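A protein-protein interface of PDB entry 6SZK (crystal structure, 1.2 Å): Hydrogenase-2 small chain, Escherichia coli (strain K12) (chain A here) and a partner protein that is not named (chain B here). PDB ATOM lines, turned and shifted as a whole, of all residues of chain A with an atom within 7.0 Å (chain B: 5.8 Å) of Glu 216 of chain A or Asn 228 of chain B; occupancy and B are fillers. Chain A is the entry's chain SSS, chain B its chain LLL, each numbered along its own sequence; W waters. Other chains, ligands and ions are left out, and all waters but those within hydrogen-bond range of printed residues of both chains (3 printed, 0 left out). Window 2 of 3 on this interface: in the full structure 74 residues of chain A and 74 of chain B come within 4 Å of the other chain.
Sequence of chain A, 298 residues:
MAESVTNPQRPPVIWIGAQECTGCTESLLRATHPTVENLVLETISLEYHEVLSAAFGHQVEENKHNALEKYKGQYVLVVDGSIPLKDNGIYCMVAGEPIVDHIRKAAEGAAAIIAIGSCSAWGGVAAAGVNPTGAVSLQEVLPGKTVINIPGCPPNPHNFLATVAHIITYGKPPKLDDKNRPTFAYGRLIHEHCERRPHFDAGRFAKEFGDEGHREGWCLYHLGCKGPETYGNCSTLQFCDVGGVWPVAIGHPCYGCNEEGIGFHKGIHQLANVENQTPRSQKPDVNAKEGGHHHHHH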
ATOM      1  N   ARG A 196      13.569   8.842 -12.468  1.00  0.00           N
ATOM      2  CA  ARG A 196      15.006   9.114 -12.259  1.00  0.00           C
ATOM      3  C   ARG A 196      15.316  10.626 -12.286  1.00  0.00           C
ATOM      4  O   ARG A 196      16.479  11.027 -12.052  1.00  0.00           O
ATOM      5  CB  ARG A 196      15.883   8.358 -13.247  1.00  0.00           C
ATOM      6  CG  ARG A 196      15.616   6.846 -13.196  1.00  0.00           C
ATOM      7  CD  ARG A 196      16.672   5.986 -13.861  1.00  0.00           C
ATOM      8  NE  ARG A 196      16.358   4.576 -13.636  1.00  0.00           N
ATOM      9  CZ  ARG A 196      17.206   3.572 -13.790  1.00  0.00           C
ATOM     10  NH1 ARG A 196      18.432   3.783 -14.275  1.00  0.00           N
ATOM     11  NH2 ARG A 196      16.837   2.335 -13.507  1.00  0.00           N
ATOM     12  N   HIS A 199      17.742  11.993  -9.572  1.00  0.00           N
ATOM     13  CA  HIS A 199      19.152  11.739  -9.850  1.00  0.00           C
ATOM     14  C   HIS A 199      19.710  12.796 -10.864  1.00  0.00           C
ATOM     15  O   HIS A 199      20.785  13.376 -10.648  1.00  0.00           O
ATOM     16  CB  HIS A 199      19.377  10.300 -10.336  1.00  0.00           C
ATOM     17  CG  HIS A 199      18.817   9.299  -9.371  1.00  0.00           C
ATOM     18  ND1 HIS A 199      19.190   9.298  -8.032  1.00  0.00           N
ATOM     19  CD2 HIS A 199      17.861   8.310  -9.528  1.00  0.00           C
ATOM     20  CE1 HIS A 199      18.490   8.327  -7.439  1.00  0.00           C
ATOM     21  NE2 HIS A 199      17.675   7.704  -8.316  1.00  0.00           N
ATOM     22  N   ASP A 211      28.728   0.388 -14.555  1.00  0.00           N
ATOM     23  CA  ASP A 211      29.473   1.210 -13.567  1.00  0.00           C
ATOM     24  C   ASP A 211      28.672   1.321 -12.249  1.00  0.00           C
ATOM     25  O   ASP A 211      27.517   0.819 -12.135  1.00  0.00           O
ATOM     26  CB  ASP A 211      29.997   2.522 -14.126  1.00  0.00           C
ATOM     27  CG  ASP A 211      29.001   3.684 -14.231  1.00  0.00           C
ATOM     28  OD1 ASP A 211      27.804   3.578 -13.800  1.00  0.00           O
ATOM     29  OD2 ASP A 211      29.450   4.769 -14.745  1.00  0.00           O
ATOM     30  N   GLU A 212      29.248   1.956 -11.229  1.00  0.00           N
ATOM     31  CA  GLU A 212      28.631   1.894  -9.873  1.00  0.00           C
ATOM     32  C   GLU A 212      27.310   2.662  -9.895  1.00  0.00           C
ATOM     33  O   GLU A 212      26.297   2.158  -9.325  1.00  0.00           O
ATOM     34  CB  GLU A 212      29.620   2.425  -8.825  1.00  0.00           C
ATOM     35  CG  GLU A 212      29.249   2.338  -7.373  1.00  0.00           C
ATOM     36  CD  GLU A 212      30.339   2.933  -6.472  1.00  0.00           C
ATOM     37  OE1 GLU A 212      31.538   2.822  -6.826  1.00  0.00           O
ATOM     38  OE2 GLU A 212      29.967   3.479  -5.388  1.00  0.00           O
ATOM     39  N   GLY A 213      27.246   3.838 -10.521  1.00  0.00           N
ATOM     40  CA  GLY A 213      25.966   4.594 -10.582  1.00  0.00           C
ATOM     41  C   GLY A 213      24.896   3.908 -11.390  1.00  0.00           C
ATOM     42  O   GLY A 213      23.692   3.893 -11.002  1.00  0.00           O
ATOM     43  N   HIS A 214      25.294   3.296 -12.518  1.00  0.00           N
ATOM     44  CA  HIS A 214      24.354   2.463 -13.320  1.00  0.00           C
ATOM     45  C   HIS A 214      23.727   1.352 -12.420  1.00  0.00           C
ATOM     46  O   HIS A 214      22.471   1.108 -12.498  1.00  0.00           O
ATOM     47  CB  HIS A 214      25.080   1.910 -14.537  1.00  0.00           C
ATOM     48  CG  HIS A 214      24.204   1.184 -15.504  1.00  0.00           C
ATOM     49  ND1 HIS A 214      24.433  -0.147 -15.819  1.00  0.00           N
ATOM     50  CD2 HIS A 214      23.127   1.618 -16.257  1.00  0.00           C
ATOM     51  CE1 HIS A 214      23.525  -0.516 -16.697  1.00  0.00           C
ATOM     52  NE2 HIS A 214      22.675   0.528 -16.997  1.00  0.00           N
ATOM     53  N   ARG A 215      24.583   0.691 -11.610  1.00  0.00           N
ATOM     54  CA  ARG A 215      24.155  -0.407 -10.732  1.00  0.00           C
ATOM     55  C   ARG A 215      23.412   0.094  -9.462  1.00  0.00           C
ATOM     56  O   ARG A 215      22.960  -0.764  -8.687  1.00  0.00           O
ATOM     57  CB  ARG A 215      25.352  -1.305 -10.409  1.00  0.00           C
ATOM     58  CG  ARG A 215      25.849  -2.101 -11.639  1.00  0.00           C
ATOM     59  CD  ARG A 215      27.106  -2.927 -11.403  1.00  0.00           C
ATOM     60  NE  ARG A 215      26.852  -3.933 -10.455  1.00  0.00           N
ATOM     61  CZ  ARG A 215      27.345  -3.997  -9.207  1.00  0.00           C
ATOM     62  NH1 ARG A 215      28.348  -3.201  -8.814  1.00  0.00           N
ATOM     63  NH2 ARG A 215      26.838  -4.972  -8.403  1.00  0.00           N
ATOM     64  N   GLU A 216      23.210   1.428  -9.328  1.00  0.00           N
ATOM     65  CA  GLU A 216      22.339   1.999  -8.324  1.00  0.00           C
ATOM     66  C   GLU A 216      21.074   2.638  -8.933  1.00  0.00           C
ATOM     67  O   GLU A 216      20.281   3.270  -8.186  1.00  0.00           O
ATOM     68  CB  GLU A 216      23.101   3.002  -7.425  1.00  0.00           C
ATOM     69  CG  GLU A 216      24.232   2.365  -6.670  1.00  0.00           C
ATOM     70  CD  GLU A 216      23.907   1.305  -5.602  1.00  0.00           C
ATOM     71  OE1 GLU A 216      22.747   1.204  -5.107  1.00  0.00           O
ATOM     72  OE2 GLU A 216      24.837   0.484  -5.250  1.00  0.00           O
ATOM     73  N   GLY A 217      20.838   2.497 -10.232  1.00  0.00           N
ATOM     74  CA  GLY A 217      19.614   3.055 -10.866  1.00  0.00           C
ATOM     75  C   GLY A 217      19.613   4.562 -11.048  1.00  0.00           C
ATOM     76  O   GLY A 217      18.539   5.184 -11.074  1.00  0.00           O
ATOM     77  N   TRP A 218      20.784   5.150 -11.286  1.00  0.00           N
ATOM     78  CA  TRP A 218      20.916   6.606 -11.505  1.00  0.00           C
ATOM     79  C   TRP A 218      20.434   7.020 -12.909  1.00  0.00           C
ATOM     80  O   TRP A 218      20.083   6.183 -13.801  1.00  0.00           O
ATOM     81  CB  TRP A 218      22.369   7.029 -11.240  1.00  0.00           C
ATOM     82  CG  TRP A 218      22.792   7.033  -9.804  1.00  0.00           C
ATOM     83  CD1 TRP A 218      22.071   6.647  -8.702  1.00  0.00           C
ATOM     84  CD2 TRP A 218      24.102   7.399  -9.264  1.00  0.00           C
ATOM     85  NE1 TRP A 218      22.842   6.780  -7.551  1.00  0.00           N
ATOM     86  CE2 TRP A 218      24.060   7.275  -7.879  1.00  0.00           C
ATOM     87  CE3 TRP A 218      25.275   7.892  -9.868  1.00  0.00           C
ATOM     88  CZ2 TRP A 218      25.143   7.652  -7.068  1.00  0.00           C
ATOM     89  CZ3 TRP A 218      26.359   8.245  -9.101  1.00  0.00           C
ATOM     90  CH2 TRP A 218      26.288   8.092  -7.715  1.00  0.00           C
ATOM     91  N   PRO B 226      21.722  -3.874 -15.217  1.00  0.00           N
ATOM     92  CA  PRO B 226      22.706  -3.679 -14.140  1.00  0.00           C
ATOM     93  C   PRO B 226      22.464  -4.754 -13.059  1.00  0.00           C
ATOM     94  O   PRO B 226      21.422  -4.726 -12.356  1.00  0.00           O
ATOM     95  CB  PRO B 226      22.412  -2.278 -13.582  1.00  0.00           C
ATOM     96  CG  PRO B 226      21.109  -1.794 -14.256  1.00  0.00           C
ATOM     97  CD  PRO B 226      20.520  -3.004 -14.967  1.00  0.00           C
ATOM     98  N   ILE B 227      23.407  -5.704 -12.929  1.00  0.00           N
ATOM     99  CA  ILE B 227      23.261  -6.791 -11.969  1.00  0.00           C
ATOM    100  C   ILE B 227      23.718  -6.310 -10.582  1.00  0.00           C
ATOM    101  O   ILE B 227      24.882  -5.953 -10.361  1.00  0.00           O
ATOM    102  CB  ILE B 227      24.068  -8.081 -12.380  1.00  0.00           C
ATOM    103  CG1 ILE B 227      23.464  -8.700 -13.660  1.00  0.00           C
ATOM    104  CG2 ILE B 227      24.062  -9.062 -11.228  1.00  0.00           C
ATOM    105  CD1 ILE B 227      24.241  -9.857 -14.278  1.00  0.00           C
ATOM    106  N   ASN B 228      22.776  -6.327  -9.613  1.00  0.00           N
ATOM    107  CA  ASN B 228      23.110  -5.966  -8.198  1.00  0.00           C
ATOM    108  C   ASN B 228      21.984  -6.524  -7.324  1.00  0.00           C
ATOM    109  O   ASN B 228      20.903  -5.959  -7.192  1.00  0.00           O
ATOM    110  CB  ASN B 228      23.209  -4.443  -8.047  1.00  0.00           C
ATOM    111  CG  ASN B 228      23.592  -3.969  -6.650  1.00  0.00           C
ATOM    112  OD1 ASN B 228      23.757  -4.845  -5.738  1.00  0.00           O
ATOM    113  ND2 ASN B 228      23.727  -2.659  -6.480  1.00  0.00           N
ATOM    114  N   LEU B 229      22.298  -7.670  -6.698  1.00  0.00           N
ATOM    115  CA  LEU B 229      21.264  -8.320  -5.844  1.00  0.00           C
ATOM    116  C   LEU B 229      20.758  -7.403  -4.726  1.00  0.00           C
ATOM    117  O   LEU B 229      19.568  -7.621  -4.279  1.00  0.00           O
ATOM    118  CB  LEU B 229      21.733  -9.646  -5.226  1.00  0.00           C
ATOM    119  CG  LEU B 229      22.136 -10.747  -6.210  1.00  0.00           C
ATOM    120  CD1 LEU B 229      22.312 -12.067  -5.484  1.00  0.00           C
ATOM    121  CD2 LEU B 229      21.055 -10.973  -7.280  1.00  0.00           C
ATOM    122  N   ASP B 230      21.551  -6.425  -4.258  1.00  0.00           N
ATOM    123  CA  ASP B 230      21.194  -5.552  -3.143  1.00  0.00           C
ATOM    124  C   ASP B 230      20.756  -4.156  -3.587  1.00  0.00           C
ATOM    125  O   ASP B 230      20.579  -3.278  -2.719  1.00  0.00           O
ATOM    126  CB  ASP B 230      22.381  -5.535  -2.185  1.00  0.00           C
ATOM    127  CG  ASP B 230      22.601  -6.939  -1.565  1.00  0.00           C
ATOM    128  OD1 ASP B 230      21.679  -7.472  -0.872  1.00  0.00           O
ATOM    129  OD2 ASP B 230      23.705  -7.514  -1.802  1.00  0.00           O
ATOM    130  N   GLY B 231      20.571  -3.941  -4.901  1.00  0.00           N
ATOM    131  CA  GLY B 231      20.202  -2.630  -5.427  1.00  0.00           C
ATOM    132  C   GLY B 231      18.712  -2.392  -5.639  1.00  0.00           C
ATOM    133  O   GLY B 231      18.021  -3.242  -6.091  1.00  0.00           O
ATOM    134  N   LEU B 232      18.285  -1.165  -5.348  1.00  0.00           N
ATOM    135  CA  LEU B 232      16.911  -0.679  -5.615  1.00  0.00           C
ATOM    136  C   LEU B 232      16.881  -0.215  -7.078  1.00  0.00           C
ATOM    137  O   LEU B 232      17.807   0.490  -7.543  1.00  0.00           O
ATOM    138  CB  LEU B 232      16.551   0.408  -4.589  1.00  0.00           C
ATOM    139  CG  LEU B 232      15.110   0.943  -4.587  1.00  0.00           C
ATOM    140  CD1 LEU B 232      14.734   1.382  -3.190  1.00  0.00           C
ATOM    141  CD2 LEU B 232      14.978   2.083  -5.593  1.00  0.00           C
ATOM    142  N   VAL B 234      17.200  -1.870  -9.979  1.00  0.00           N
ATOM    143  CA  VAL B 234      18.070  -2.611 -10.912  1.00  0.00           C
ATOM    144  C   VAL B 234      17.726  -4.109 -10.904  1.00  0.00           C
ATOM    145  O   VAL B 234      16.707  -4.550 -10.327  1.00  0.00           O
ATOM    146  CB  VAL B 234      19.570  -2.282 -10.616  1.00  0.00           C
ATOM    147  CG1 VAL B 234      19.826  -0.767 -10.687  1.00  0.00           C
ATOM    148  CG2 VAL B 234      19.991  -2.785  -9.250  1.00  0.00           C
ATOM    149  N   LEU B 235      18.560  -4.927 -11.577  1.00  0.00           N
ATOM    150  CA  LEU B 235      18.323  -6.408 -11.712  1.00  0.00           C
ATOM    151  C   LEU B 235      18.810  -7.058 -10.419  1.00  0.00           C
ATOM    152  O   LEU B 235      19.997  -7.410 -10.258  1.00  0.00           O
ATOM    153  CB  LEU B 235      18.982  -6.954 -12.985  1.00  0.00           C
ATOM    154  CG  LEU B 235      18.672  -8.450 -13.277  1.00  0.00           C
ATOM    155  CD1 LEU B 235      17.149  -8.686 -13.398  1.00  0.00           C
ATOM    156  CD2 LEU B 235      19.376  -8.906 -14.534  1.00  0.00           C
ATOM    157  N   ASN B 236      17.854  -7.192  -9.462  1.00  0.00           N
ATOM    158  CA  ASN B 236      18.127  -7.739  -8.111  1.00  0.00           C
ATOM    159  C   ASN B 236      17.483  -9.135  -7.947  1.00  0.00           C
ATOM    160  O   ASN B 236      16.953  -9.716  -8.939  1.00  0.00           O
ATOM    161  CB  ASN B 236      17.724  -6.689  -7.021  1.00  0.00           C
ATOM    162  CG  ASN B 236      16.200  -6.383  -7.067  1.00  0.00           C
ATOM    163  OD1 ASN B 236      15.425  -7.265  -7.501  1.00  0.00           O
ATOM    164  ND2 ASN B 236      15.800  -5.151  -6.665  1.00  0.00           N
ATOM    165  N   LEU B 237      17.517  -9.734  -6.744  1.00  0.00           N
ATOM    166  CA  LEU B 237      16.990 -11.104  -6.574  1.00  0.00           C
ATOM    167  C   LEU B 237      15.482 -11.136  -6.767  1.00  0.00           C
ATOM    168  O   LEU B 237      14.964 -12.109  -7.343  1.00  0.00           O
ATOM    169  CB  LEU B 237      17.449 -11.693  -5.226  1.00  0.00           C
ATOM    170  CG  LEU B 237      17.166 -13.212  -5.060  1.00  0.00           C
ATOM    171  CD1 LEU B 237      17.767 -14.073  -6.181  1.00  0.00           C
ATOM    172  CD2 LEU B 237      17.634 -13.654  -3.686  1.00  0.00           C
ATOM    173  N   HIS B 455      29.419  -9.788 -11.179  1.00  0.00           N
ATOM    174  CA  HIS B 455      28.294  -8.903 -11.589  1.00  0.00           C
ATOM    175  C   HIS B 455      28.591  -8.183 -12.905  1.00  0.00           C
ATOM    176  O   HIS B 455      27.842  -7.271 -13.260  1.00  0.00           O
ATOM    177  CB  HIS B 455      27.920  -7.917 -10.458  1.00  0.00           C
ATOM    178  CG  HIS B 455      29.062  -6.979 -10.115  1.00  0.00           C
ATOM    179  ND1 HIS B 455      29.783  -7.047  -8.926  1.00  0.00           N
ATOM    180  CD2 HIS B 455      29.657  -6.004 -10.812  1.00  0.00           C
ATOM    181  CE1 HIS B 455      30.766  -6.142  -8.914  1.00  0.00           C
ATOM    182  NE2 HIS B 455      30.721  -5.500 -10.098  1.00  0.00           N
HETATM  183  O   HOH W   1      19.983   1.372  -5.559  1.00  0.00           O
HETATM  184  O   HOH W   2      24.531  -1.453  -3.842  1.00  0.00           O
HETATM  185  O   HOH W   3      22.274  -0.487  -2.876  1.00  0.00           O
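The side-chain amide oxygen of Asn 228 of chain B is in hydrogen-bond range of the backbone NH of Gly 231 of chain B, at 3.4 Å.
O of Pro 226 of chain B lies within hydrogen-bond range of N of Leu 235 of chain B (3.0 Å).
The backbone NH (N) of Asp 230 of chain B sits at hydrogen-bond distance from the side-chain amide oxygen (OD1) of Asn 228 of chain B (3.1 Å).
The guanidinium group of Arg 196 of chain A lies within hydrogen-bond range of the backbone carbonyl oxygen of Gly 217 of chain A, 3.4 Å away.
The backbone carbonyl oxygen (O) of Leu 235 of chain B sits at hydrogen-bond distance from the backbone NH (N) of Asn 228 of chain B (3.1 Å).
The backbone NH (N) of His 214 of chain A sits at hydrogen-bond distance from the side-chain carboxylate (OD1) of Asp 211 of chain A (2.8 Å).
Water W2 lies within hydrogen-bond range of OE2 of Glu 216 of chain A and ND2 of Asn 228 of chain B.
Water W1 bridges the side-chain carboxylate of Glu 216 of chain A (2.8 Å) and the backbone NH of Leu 232 of chain B (3.1 Å).
Water W3 bridges the side-chain carboxylate of Glu 216 of chain A (2.8 Å) and the backbone carbonyl oxygen of Asp 230 of chain B (3.3 Å).
Glu 212 of chain A touches none of the printed residues of chain B.
Glu 216 of chain A touches just these residues of chain B: Asn 228 (3.6 Å) and Leu 232 (3.8 Å).
Printed residues of chain A within 4 Å of Ile 227 of chain B: Arg 215.
Of chain A, only Arg 215 (3.0 Å) and Glu 216 (3.6 Å) come within 4 Å of Asn 228 of chain B.
Of the printed residues of chain A, Val 234 of chain B touches His 214 (3.7 Å), Arg 215 (3.6 Å) and Gly 217 (3.4 Å).
Leu 235 of chain B touches none of the printed residues of chain A.
The nearest residue of chain B that does not touch Glu 216 of chain A is Val 234 of chain B (4.03 Å).
The nearest printed residue of chain A that does not touch Pro 226 of chain B is Glu 216 of chain A (5.7 Å).
O of Ile 227 of chain B sits at hydrogen-bond distance from NE of Arg 215 of chain A.
O of Arg 215 of chain A sits at hydrogen-bond distance from ND2 of Asn 228 of chain B, 3.0 Å away.
Along chain A the printed residues that touch a printed residue of chain B span positions 214 to 217.
Of the 12 printed residues of chain B, 6 touch a printed residue of chain A.
Printed residues of chain B that touch a printed residue of chain A: Pro 226, Ile 227, Asn 228, Leu 232, Val 234 and His 455.
Among the printed residues, 10 pairs touch across the chains.
Pro 226 of chain B touches His 214 of chain A (CB to O, 3.6 Å).
Val 234 of chain B touches His 214 of chain A.
CB of Pro 226 of chain B touches CA of Arg 215 of chain A, at 3.8 Å.
Arg 215 of chain A touches Val 234 of chain B (O to CG2, 3.6 Å).
CG of His 455 of chain B touches NH2 of Arg 215 of chain A (3.5 Å).
OE2 of Glu 216 of chain A touches ND2 of Asn 228 of chain B, 3.6 Å away.
Leu 232 of chain B touches Glu 216 of chain A (O to O, 3.8 Å).
Val 234 of chain B touches Gly 217 of chain A (CG1 to N, 3.4 Å).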
